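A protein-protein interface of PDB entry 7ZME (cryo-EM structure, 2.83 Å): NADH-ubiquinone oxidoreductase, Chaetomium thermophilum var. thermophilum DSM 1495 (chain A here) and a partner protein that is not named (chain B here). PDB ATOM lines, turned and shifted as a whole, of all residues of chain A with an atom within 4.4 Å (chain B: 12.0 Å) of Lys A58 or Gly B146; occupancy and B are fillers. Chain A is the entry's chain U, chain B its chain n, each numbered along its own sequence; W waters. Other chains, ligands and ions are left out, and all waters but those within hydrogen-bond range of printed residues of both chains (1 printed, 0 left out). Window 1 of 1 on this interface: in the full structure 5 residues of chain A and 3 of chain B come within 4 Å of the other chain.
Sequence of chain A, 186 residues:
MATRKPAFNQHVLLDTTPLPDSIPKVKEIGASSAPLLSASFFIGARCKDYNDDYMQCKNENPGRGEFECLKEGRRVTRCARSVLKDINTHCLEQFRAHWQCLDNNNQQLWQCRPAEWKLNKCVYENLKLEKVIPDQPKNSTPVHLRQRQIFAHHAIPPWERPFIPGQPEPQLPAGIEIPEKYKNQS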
ATOM      1  N   TYR A  54      39.687 -17.973   1.658  1.00  0.00           N
ATOM      2  CA  TYR A  54      39.386 -16.558   1.990  1.00  0.00           C
ATOM      3  C   TYR A  54      37.971 -16.213   1.510  1.00  0.00           C
ATOM      4  O   TYR A  54      37.293 -15.433   2.196  1.00  0.00           O
ATOM      5  CB  TYR A  54      40.434 -15.664   1.327  1.00  0.00           C
ATOM      6  CG  TYR A  54      40.149 -14.185   1.314  1.00  0.00           C
ATOM      7  CD1 TYR A  54      40.138 -13.450   2.486  1.00  0.00           C
ATOM      8  CD2 TYR A  54      39.910 -13.515   0.126  1.00  0.00           C
ATOM      9  CE1 TYR A  54      39.887 -12.090   2.483  1.00  0.00           C
ATOM     10  CE2 TYR A  54      39.655 -12.156   0.104  1.00  0.00           C
ATOM     11  CZ  TYR A  54      39.648 -11.441   1.287  1.00  0.00           C
ATOM     12  OH  TYR A  54      39.400 -10.101   1.286  1.00  0.00           O
ATOM     13  N   MET A  55      37.536 -16.788   0.394  1.00  0.00           N
ATOM     14  CA  MET A  55      36.197 -16.513  -0.194  1.00  0.00           C
ATOM     15  C   MET A  55      35.086 -17.153   0.637  1.00  0.00           C
ATOM     16  O   MET A  55      34.008 -16.554   0.722  1.00  0.00           O
ATOM     17  CB  MET A  55      36.149 -16.966  -1.656  1.00  0.00           C
ATOM     18  CG  MET A  55      37.138 -16.239  -2.540  1.00  0.00           C
ATOM     19  SD  MET A  55      36.832 -14.465  -2.655  1.00  0.00           S
ATOM     20  CE  MET A  55      35.448 -14.432  -3.790  1.00  0.00           C
ATOM     21  N   GLN A  56      35.350 -18.332   1.203  1.00  0.00           N
ATOM     22  CA  GLN A  56      34.369 -19.049   2.058  1.00  0.00           C
ATOM     23  C   GLN A  56      34.357 -18.372   3.427  1.00  0.00           C
ATOM     24  O   GLN A  56      33.303 -18.415   4.075  1.00  0.00           O
ATOM     25  CB  GLN A  56      34.762 -20.513   2.211  1.00  0.00           C
ATOM     26  CG  GLN A  56      34.608 -21.344   0.948  1.00  0.00           C
ATOM     27  CD  GLN A  56      35.355 -22.648   1.074  1.00  0.00           C
ATOM     28  OE1 GLN A  56      35.169 -23.572   0.288  1.00  0.00           O
ATOM     29  NE2 GLN A  56      36.212 -22.733   2.077  1.00  0.00           N
ATOM     30  N   CYS A  57      35.465 -17.747   3.839  1.00  0.00           N
ATOM     31  CA  CYS A  57      35.420 -16.971   5.073  1.00  0.00           C
ATOM     32  C   CYS A  57      34.481 -15.782   4.936  1.00  0.00           C
ATOM     33  O   CYS A  57      33.657 -15.521   5.817  1.00  0.00           O
ATOM     34  CB  CYS A  57      36.829 -16.503   5.443  1.00  0.00           C
ATOM     35  SG  CYS A  57      36.935 -15.439   6.900  1.00  0.00           S
ATOM     36  N   LYS A  58      34.598 -15.044   3.831  1.00  0.00           N
ATOM     37  CA  LYS A  58      33.768 -13.860   3.644  1.00  0.00           C
ATOM     38  C   LYS A  58      32.298 -14.230   3.532  1.00  0.00           C
ATOM     39  O   LYS A  58      31.434 -13.519   4.055  1.00  0.00           O
ATOM     40  CB  LYS A  58      34.233 -13.085   2.417  1.00  0.00           C
ATOM     41  CG  LYS A  58      35.549 -12.370   2.625  1.00  0.00           C
ATOM     42  CD  LYS A  58      36.027 -11.712   1.358  1.00  0.00           C
ATOM     43  CE  LYS A  58      35.579 -10.269   1.291  1.00  0.00           C
ATOM     44  NZ  LYS A  58      36.280  -9.549   0.196  1.00  0.00           N
ATOM     45  N   ASN A  59      31.996 -15.343   2.860  1.00  0.00           N
ATOM     46  CA  ASN A  59      30.625 -15.829   2.782  1.00  0.00           C
ATOM     47  C   ASN A  59      30.096 -16.297   4.130  1.00  0.00           C
ATOM     48  O   ASN A  59      28.878 -16.374   4.310  1.00  0.00           O
ATOM     49  CB  ASN A  59      30.535 -16.965   1.770  1.00  0.00           C
ATOM     50  CG  ASN A  59      30.286 -16.473   0.373  1.00  0.00           C
ATOM     51  OD1 ASN A  59      30.521 -15.309   0.066  1.00  0.00           O
ATOM     52  ND2 ASN A  59      29.808 -17.357  -0.490  1.00  0.00           N
ATOM     53  N   GLU A  60      30.980 -16.609   5.073  1.00  0.00           N
ATOM     54  CA  GLU A  60      30.588 -17.014   6.414  1.00  0.00           C
ATOM     55  C   GLU A  60      30.425 -15.826   7.352  1.00  0.00           C
ATOM     56  O   GLU A  60      29.903 -15.989   8.458  1.00  0.00           O
ATOM     57  CB  GLU A  60      31.625 -18.001   6.966  1.00  0.00           C
ATOM     58  CG  GLU A  60      31.328 -18.605   8.325  1.00  0.00           C
ATOM     59  CD  GLU A  60      32.398 -19.585   8.757  1.00  0.00           C
ATOM     60  OE1 GLU A  60      33.374 -19.762   7.999  1.00  0.00           O
ATOM     61  OE2 GLU A  60      32.264 -20.176   9.850  1.00  0.00           O
ATOM     62  N   ASN A  61      30.821 -14.633   6.920  1.00  0.00           N
ATOM     63  CA  ASN A  61      30.602 -13.391   7.660  1.00  0.00           C
ATOM     64  C   ASN A  61      29.953 -12.381   6.724  1.00  0.00           C
ATOM     65  O   ASN A  61      30.589 -11.406   6.307  1.00  0.00           O
ATOM     66  CB  ASN A  61      31.913 -12.845   8.224  1.00  0.00           C
ATOM     67  CG  ASN A  61      32.492 -13.724   9.307  1.00  0.00           C
ATOM     68  OD1 ASN A  61      33.311 -14.599   9.036  1.00  0.00           O
ATOM     69  ND2 ASN A  61      32.077 -13.490  10.544  1.00  0.00           N
ATOM     70  N   PRO A  62      28.687 -12.589   6.367  1.00  0.00           N
ATOM     71  CA  PRO A  62      28.048 -11.717   5.372  1.00  0.00           C
ATOM     72  C   PRO A  62      27.952 -10.278   5.855  1.00  0.00           C
ATOM     73  O   PRO A  62      27.482 -10.004   6.960  1.00  0.00           O
ATOM     74  CB  PRO A  62      26.661 -12.347   5.193  1.00  0.00           C
ATOM     75  CG  PRO A  62      26.816 -13.750   5.663  1.00  0.00           C
ATOM     76  CD  PRO A  62      27.801 -13.687   6.778  1.00  0.00           C
ATOM     77  N   GLY A  63      28.401  -9.355   5.008  1.00  0.00           N
ATOM     78  CA  GLY A  63      28.359  -7.944   5.310  1.00  0.00           C
ATOM     79  C   GLY A  63      29.456  -7.462   6.223  1.00  0.00           C
ATOM     80  O   GLY A  63      29.576  -6.251   6.436  1.00  0.00           O
ATOM     81  N   GLY A  65      32.701  -9.516   6.438  1.00  0.00           N
ATOM     82  CA  GLY A  65      33.892 -10.294   6.150  1.00  0.00           C
ATOM     83  C   GLY A  65      35.108  -9.484   5.760  1.00  0.00           C
ATOM     84  O   GLY A  65      36.209 -10.042   5.729  1.00  0.00           O
ATOM     85  N   CYS A  69      37.973 -11.174   7.938  1.00  0.00           N
ATOM     86  CA  CYS A  69      38.790 -12.206   7.240  1.00  0.00           C
ATOM     87  C   CYS A  69      40.161 -11.631   6.858  1.00  0.00           C
ATOM     88  O   CYS A  69      40.704 -12.047   5.821  1.00  0.00           O
ATOM     89  CB  CYS A  69      38.087 -12.744   5.999  1.00  0.00           C
ATOM     90  SG  CYS A  69      36.488 -13.536   6.312  1.00  0.00           S
ATOM     91  N   SER B 139      20.686 -11.782  -8.413  1.00  0.00           N
ATOM     92  CA  SER B 139      21.481 -12.198  -9.602  1.00  0.00           C
ATOM     93  C   SER B 139      22.465 -13.320  -9.279  1.00  0.00           C
ATOM     94  O   SER B 139      23.085 -13.272  -8.210  1.00  0.00           O
ATOM     95  CB  SER B 139      22.179 -11.016 -10.223  1.00  0.00           C
ATOM     96  OG  SER B 139      22.895 -11.395 -11.385  1.00  0.00           O
ATOM     97  N   PHE B 141      25.253 -13.735 -10.856  1.00  0.00           N
ATOM     98  CA  PHE B 141      26.495 -13.314 -11.538  1.00  0.00           C
ATOM     99  C   PHE B 141      27.139 -12.111 -10.882  1.00  0.00           C
ATOM    100  O   PHE B 141      26.405 -11.321 -10.292  1.00  0.00           O
ATOM    101  CB  PHE B 141      26.184 -12.831 -12.955  1.00  0.00           C
ATOM    102  CG  PHE B 141      25.305 -13.733 -13.774  1.00  0.00           C
ATOM    103  CD1 PHE B 141      25.732 -14.998 -14.134  1.00  0.00           C
ATOM    104  CD2 PHE B 141      24.057 -13.310 -14.197  1.00  0.00           C
ATOM    105  CE1 PHE B 141      24.923 -15.827 -14.889  1.00  0.00           C
ATOM    106  CE2 PHE B 141      23.247 -14.143 -14.951  1.00  0.00           C
ATOM    107  CZ  PHE B 141      23.682 -15.401 -15.289  1.00  0.00           C
ATOM    108  N   ASN B 142      28.473 -12.087 -10.872  1.00  0.00           N
ATOM    109  CA  ASN B 142      29.231 -10.921 -10.363  1.00  0.00           C
ATOM    110  C   ASN B 142      28.908 -10.731  -8.895  1.00  0.00           C
ATOM    111  O   ASN B 142      28.780  -9.587  -8.457  1.00  0.00           O
ATOM    112  CB  ASN B 142      29.005  -9.686 -11.238  1.00  0.00           C
ATOM    113  CG  ASN B 142      29.595  -9.805 -12.622  1.00  0.00           C
ATOM    114  OD1 ASN B 142      30.452 -10.649 -12.867  1.00  0.00           O
ATOM    115  ND2 ASN B 142      29.140  -8.955 -13.525  1.00  0.00           N
ATOM    116  N   VAL B 143      28.807 -11.834  -8.169  1.00  0.00           N
ATOM    117  CA  VAL B 143      28.388 -11.747  -6.745  1.00  0.00           C
ATOM    118  C   VAL B 143      29.616 -11.488  -5.888  1.00  0.00           C
ATOM    119  O   VAL B 143      30.582 -12.255  -5.995  1.00  0.00           O
ATOM    120  CB  VAL B 143      27.631 -13.014  -6.306  1.00  0.00           C
ATOM    121  CG1 VAL B 143      27.189 -12.934  -4.856  1.00  0.00           C
ATOM    122  CG2 VAL B 143      26.449 -13.311  -7.210  1.00  0.00           C
ATOM    123  N   PRO B 144      29.628 -10.419  -5.066  1.00  0.00           N
ATOM    124  CA  PRO B 144      30.723 -10.205  -4.129  1.00  0.00           C
ATOM    125  C   PRO B 144      30.677 -11.320  -3.077  1.00  0.00           C
ATOM    126  O   PRO B 144      29.606 -11.802  -2.802  1.00  0.00           O
ATOM    127  CB  PRO B 144      30.403  -8.823  -3.543  1.00  0.00           C
ATOM    128  CG  PRO B 144      29.475  -8.184  -4.546  1.00  0.00           C
ATOM    129  CD  PRO B 144      28.644  -9.337  -5.056  1.00  0.00           C
ATOM    130  N   ALA B 145      31.828 -11.736  -2.548  1.00  0.00           N
ATOM    131  CA  ALA B 145      31.831 -12.742  -1.459  1.00  0.00           C
ATOM    132  C   ALA B 145      31.328 -12.100  -0.171  1.00  0.00           C
ATOM    133  O   ALA B 145      31.840 -11.027   0.191  1.00  0.00           O
ATOM    134  CB  ALA B 145      33.199 -13.322  -1.256  1.00  0.00           C
ATOM    135  N   GLY B 146      30.376 -12.749   0.492  1.00  0.00           N
ATOM    136  CA  GLY B 146      29.802 -12.216   1.734  1.00  0.00           C
ATOM    137  C   GLY B 146      28.702 -11.231   1.446  1.00  0.00           C
ATOM    138  O   GLY B 146      28.455 -10.368   2.293  1.00  0.00           O
ATOM    139  N   PHE B 147      28.089 -11.324   0.269  1.00  0.00           N
ATOM    140  CA  PHE B 147      27.066 -10.301  -0.074  1.00  0.00           C
ATOM    141  C   PHE B 147      25.661 -10.746   0.358  1.00  0.00           C
ATOM    142  O   PHE B 147      24.989  -9.973   1.046  1.00  0.00           O
ATOM    143  CB  PHE B 147      27.157  -9.971  -1.563  1.00  0.00           C
ATOM    144  CG  PHE B 147      26.043  -9.117  -2.109  1.00  0.00           C
ATOM    145  CD1 PHE B 147      26.177  -7.742  -2.181  1.00  0.00           C
ATOM    146  CD2 PHE B 147      24.868  -9.693  -2.563  1.00  0.00           C
ATOM    147  CE1 PHE B 147      25.155  -6.961  -2.690  1.00  0.00           C
ATOM    148  CE2 PHE B 147      23.838  -8.908  -3.050  1.00  0.00           C
ATOM    149  CZ  PHE B 147      23.991  -7.546  -3.123  1.00  0.00           C
ATOM    150  N   TYR B 148      25.235 -11.936  -0.034  1.00  0.00           N
ATOM    151  CA  TYR B 148      23.882 -12.426   0.310  1.00  0.00           C
ATOM    152  C   TYR B 148      23.800 -12.743   1.804  1.00  0.00           C
ATOM    153  O   TYR B 148      24.718 -13.361   2.352  1.00  0.00           O
ATOM    154  CB  TYR B 148      23.521 -13.611  -0.585  1.00  0.00           C
ATOM    155  CG  TYR B 148      23.180 -13.256  -2.006  1.00  0.00           C
ATOM    156  CD1 TYR B 148      22.055 -12.508  -2.301  1.00  0.00           C
ATOM    157  CD2 TYR B 148      23.972 -13.680  -3.058  1.00  0.00           C
ATOM    158  CE1 TYR B 148      21.730 -12.179  -3.604  1.00  0.00           C
ATOM    159  CE2 TYR B 148      23.660 -13.361  -4.368  1.00  0.00           C
ATOM    160  CZ  TYR B 148      22.537 -12.605  -4.641  1.00  0.00           C
ATOM    161  OH  TYR B 148      22.225 -12.278  -5.925  1.00  0.00           O
ATOM    162  N   PRO B 149      22.730 -12.316   2.503  1.00  0.00           N
ATOM    163  CA  PRO B 149      22.549 -12.662   3.905  1.00  0.00           C
ATOM    164  C   PRO B 149      22.172 -14.138   4.065  1.00  0.00           C
ATOM    165  O   PRO B 149      21.555 -14.689   3.179  1.00  0.00           O
ATOM    166  CB  PRO B 149      21.431 -11.719   4.364  1.00  0.00           C
ATOM    167  CG  PRO B 149      20.662 -11.393   3.110  1.00  0.00           C
ATOM    168  CD  PRO B 149      21.675 -11.443   1.987  1.00  0.00           C
ATOM    169  N   ASN B 150      22.588 -14.755   5.166  1.00  0.00           N
ATOM    170  CA  ASN B 150      22.164 -16.151   5.422  1.00  0.00           C
ATOM    171  C   ASN B 150      20.669 -16.124   5.725  1.00  0.00           C
ATOM    172  O   ASN B 150      20.254 -15.303   6.566  1.00  0.00           O
ATOM    173  CB  ASN B 150      22.969 -16.790   6.553  1.00  0.00           C
ATOM    174  CG  ASN B 150      22.779 -18.287   6.645  1.00  0.00           C
ATOM    175  OD1 ASN B 150      22.528 -18.950   5.641  1.00  0.00           O
ATOM    176  ND2 ASN B 150      22.908 -18.829   7.844  1.00  0.00           N
ATOM    177  N   LEU B 151      19.900 -16.989   5.069  1.00  0.00           N
ATOM    178  CA  LEU B 151      18.429 -17.030   5.261  1.00  0.00           C
ATOM    179  C   LEU B 151      18.064 -18.398   5.824  1.00  0.00           C
ATOM    180  O   LEU B 151      16.956 -18.851   5.564  1.00  0.00           O
ATOM    181  CB  LEU B 151      17.742 -16.778   3.916  1.00  0.00           C
ATOM    182  CG  LEU B 151      18.078 -15.458   3.222  1.00  0.00           C
ATOM    183  CD1 LEU B 151      17.410 -15.387   1.862  1.00  0.00           C
ATOM    184  CD2 LEU B 151      17.674 -14.268   4.077  1.00  0.00           C
HETATM  185  O   HOH W   1      31.056  -9.216   3.255  1.00  0.00           O
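OD1 of Asn A59 lies within hydrogen-bond range of N of Gly B146 (2.6 Å). The backbone NH of Gly A63 sits at hydrogen-bond distance from the backbone carbonyl oxygen of Gly B146 (2.9 Å).
The side-chain hydroxyl (OH) of Tyr A54 is in hydrogen-bond range of the side-chain amino group (NZ) of Lys A58. N of Lys A58 is in hydrogen-bond range of SG of Cys A69 (3.5 Å). O of Ser B139 sits at hydrogen-bond distance from OH of Tyr B148. The side-chain sulfur of Cys A57 is disulfide-bonded to the side-chain sulfur of Cys A69 (2.0 Å).
Among the printed residues, merely in contact across the chains: Lys A58 with Gly B146 (3.1 Å), Asn A59 with Ala B145 (3.3 Å), Pro A62 with Gly B146 (3.4 Å), Met A55 with Ala B145 (3.6 Å), Pro A62 with Tyr B148 (3.6 Å) and Lys A58 with Ala B145 (3.8 Å).
Lys A58 touches just these residues of chain B: Ala B145 (3.8 Å) and Gly B146 (3.1 Å). Gly B146 touches four residues of chain A. No residue of chain B comes within 4 Å of Tyr A54. Of chain B, only Ala B145 (3.6 Å) comes within 4 Å of Met A55. No residue of chain B comes within 4 Å of Cys A57. No residue of chain B comes within 4 Å of Asn A61. Of chain B, only Gly B146 (3.4 Å) and Tyr B148 (3.6 Å) come within 4 Å of Pro A62. Of the printed residues of chain B, Gly A63 touches Gly B146 (2.9 Å). No residue of chain B comes within 4 Å of Gly A65. No residue of chain B comes within 4 Å of Cys A69. Of the printed residues of chain A, Tyr B148 touches Pro A62 (3.6 Å). Of the printed residues of chain A, Ala B145 touches Met A55, Lys A58 and Asn A59. Phe B141 touches none of the printed residues of chain A. Val B143 touches none of the printed residues of chain A. The nearest residue of chain B that does not touch Lys A58 is Phe B147 (5.5 Å).
Of the 12 printed residues of chain B, 3 touch a printed residue of chain A. Printed residues of chain B that touch a printed residue of chain A: Ala B145, Gly B146 and Tyr B148. Hydrophobic or aromatic side chains of chain B within 4 Å of the printed part of chain A: Ala B145. Along chain B the printed residues that touch a printed residue of chain A span positions 145 to 148. Of the 12 printed residues of chain A, 5 touch a printed residue of chain B. Printed residues of chain A that touch a printed residue of chain B: Met A55, Lys A58, Asn A59, Pro A62 and Gly A63. Hydrophobic or aromatic side chains of chain A that line the printed part of chain B: Met A55 and Pro A62.
Water W1 lies within hydrogen-bond range of the backbone carbonyl oxygen of Gly B146 (3.0 Å) and the backbone NH of Gly A63 (3.2 Å).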
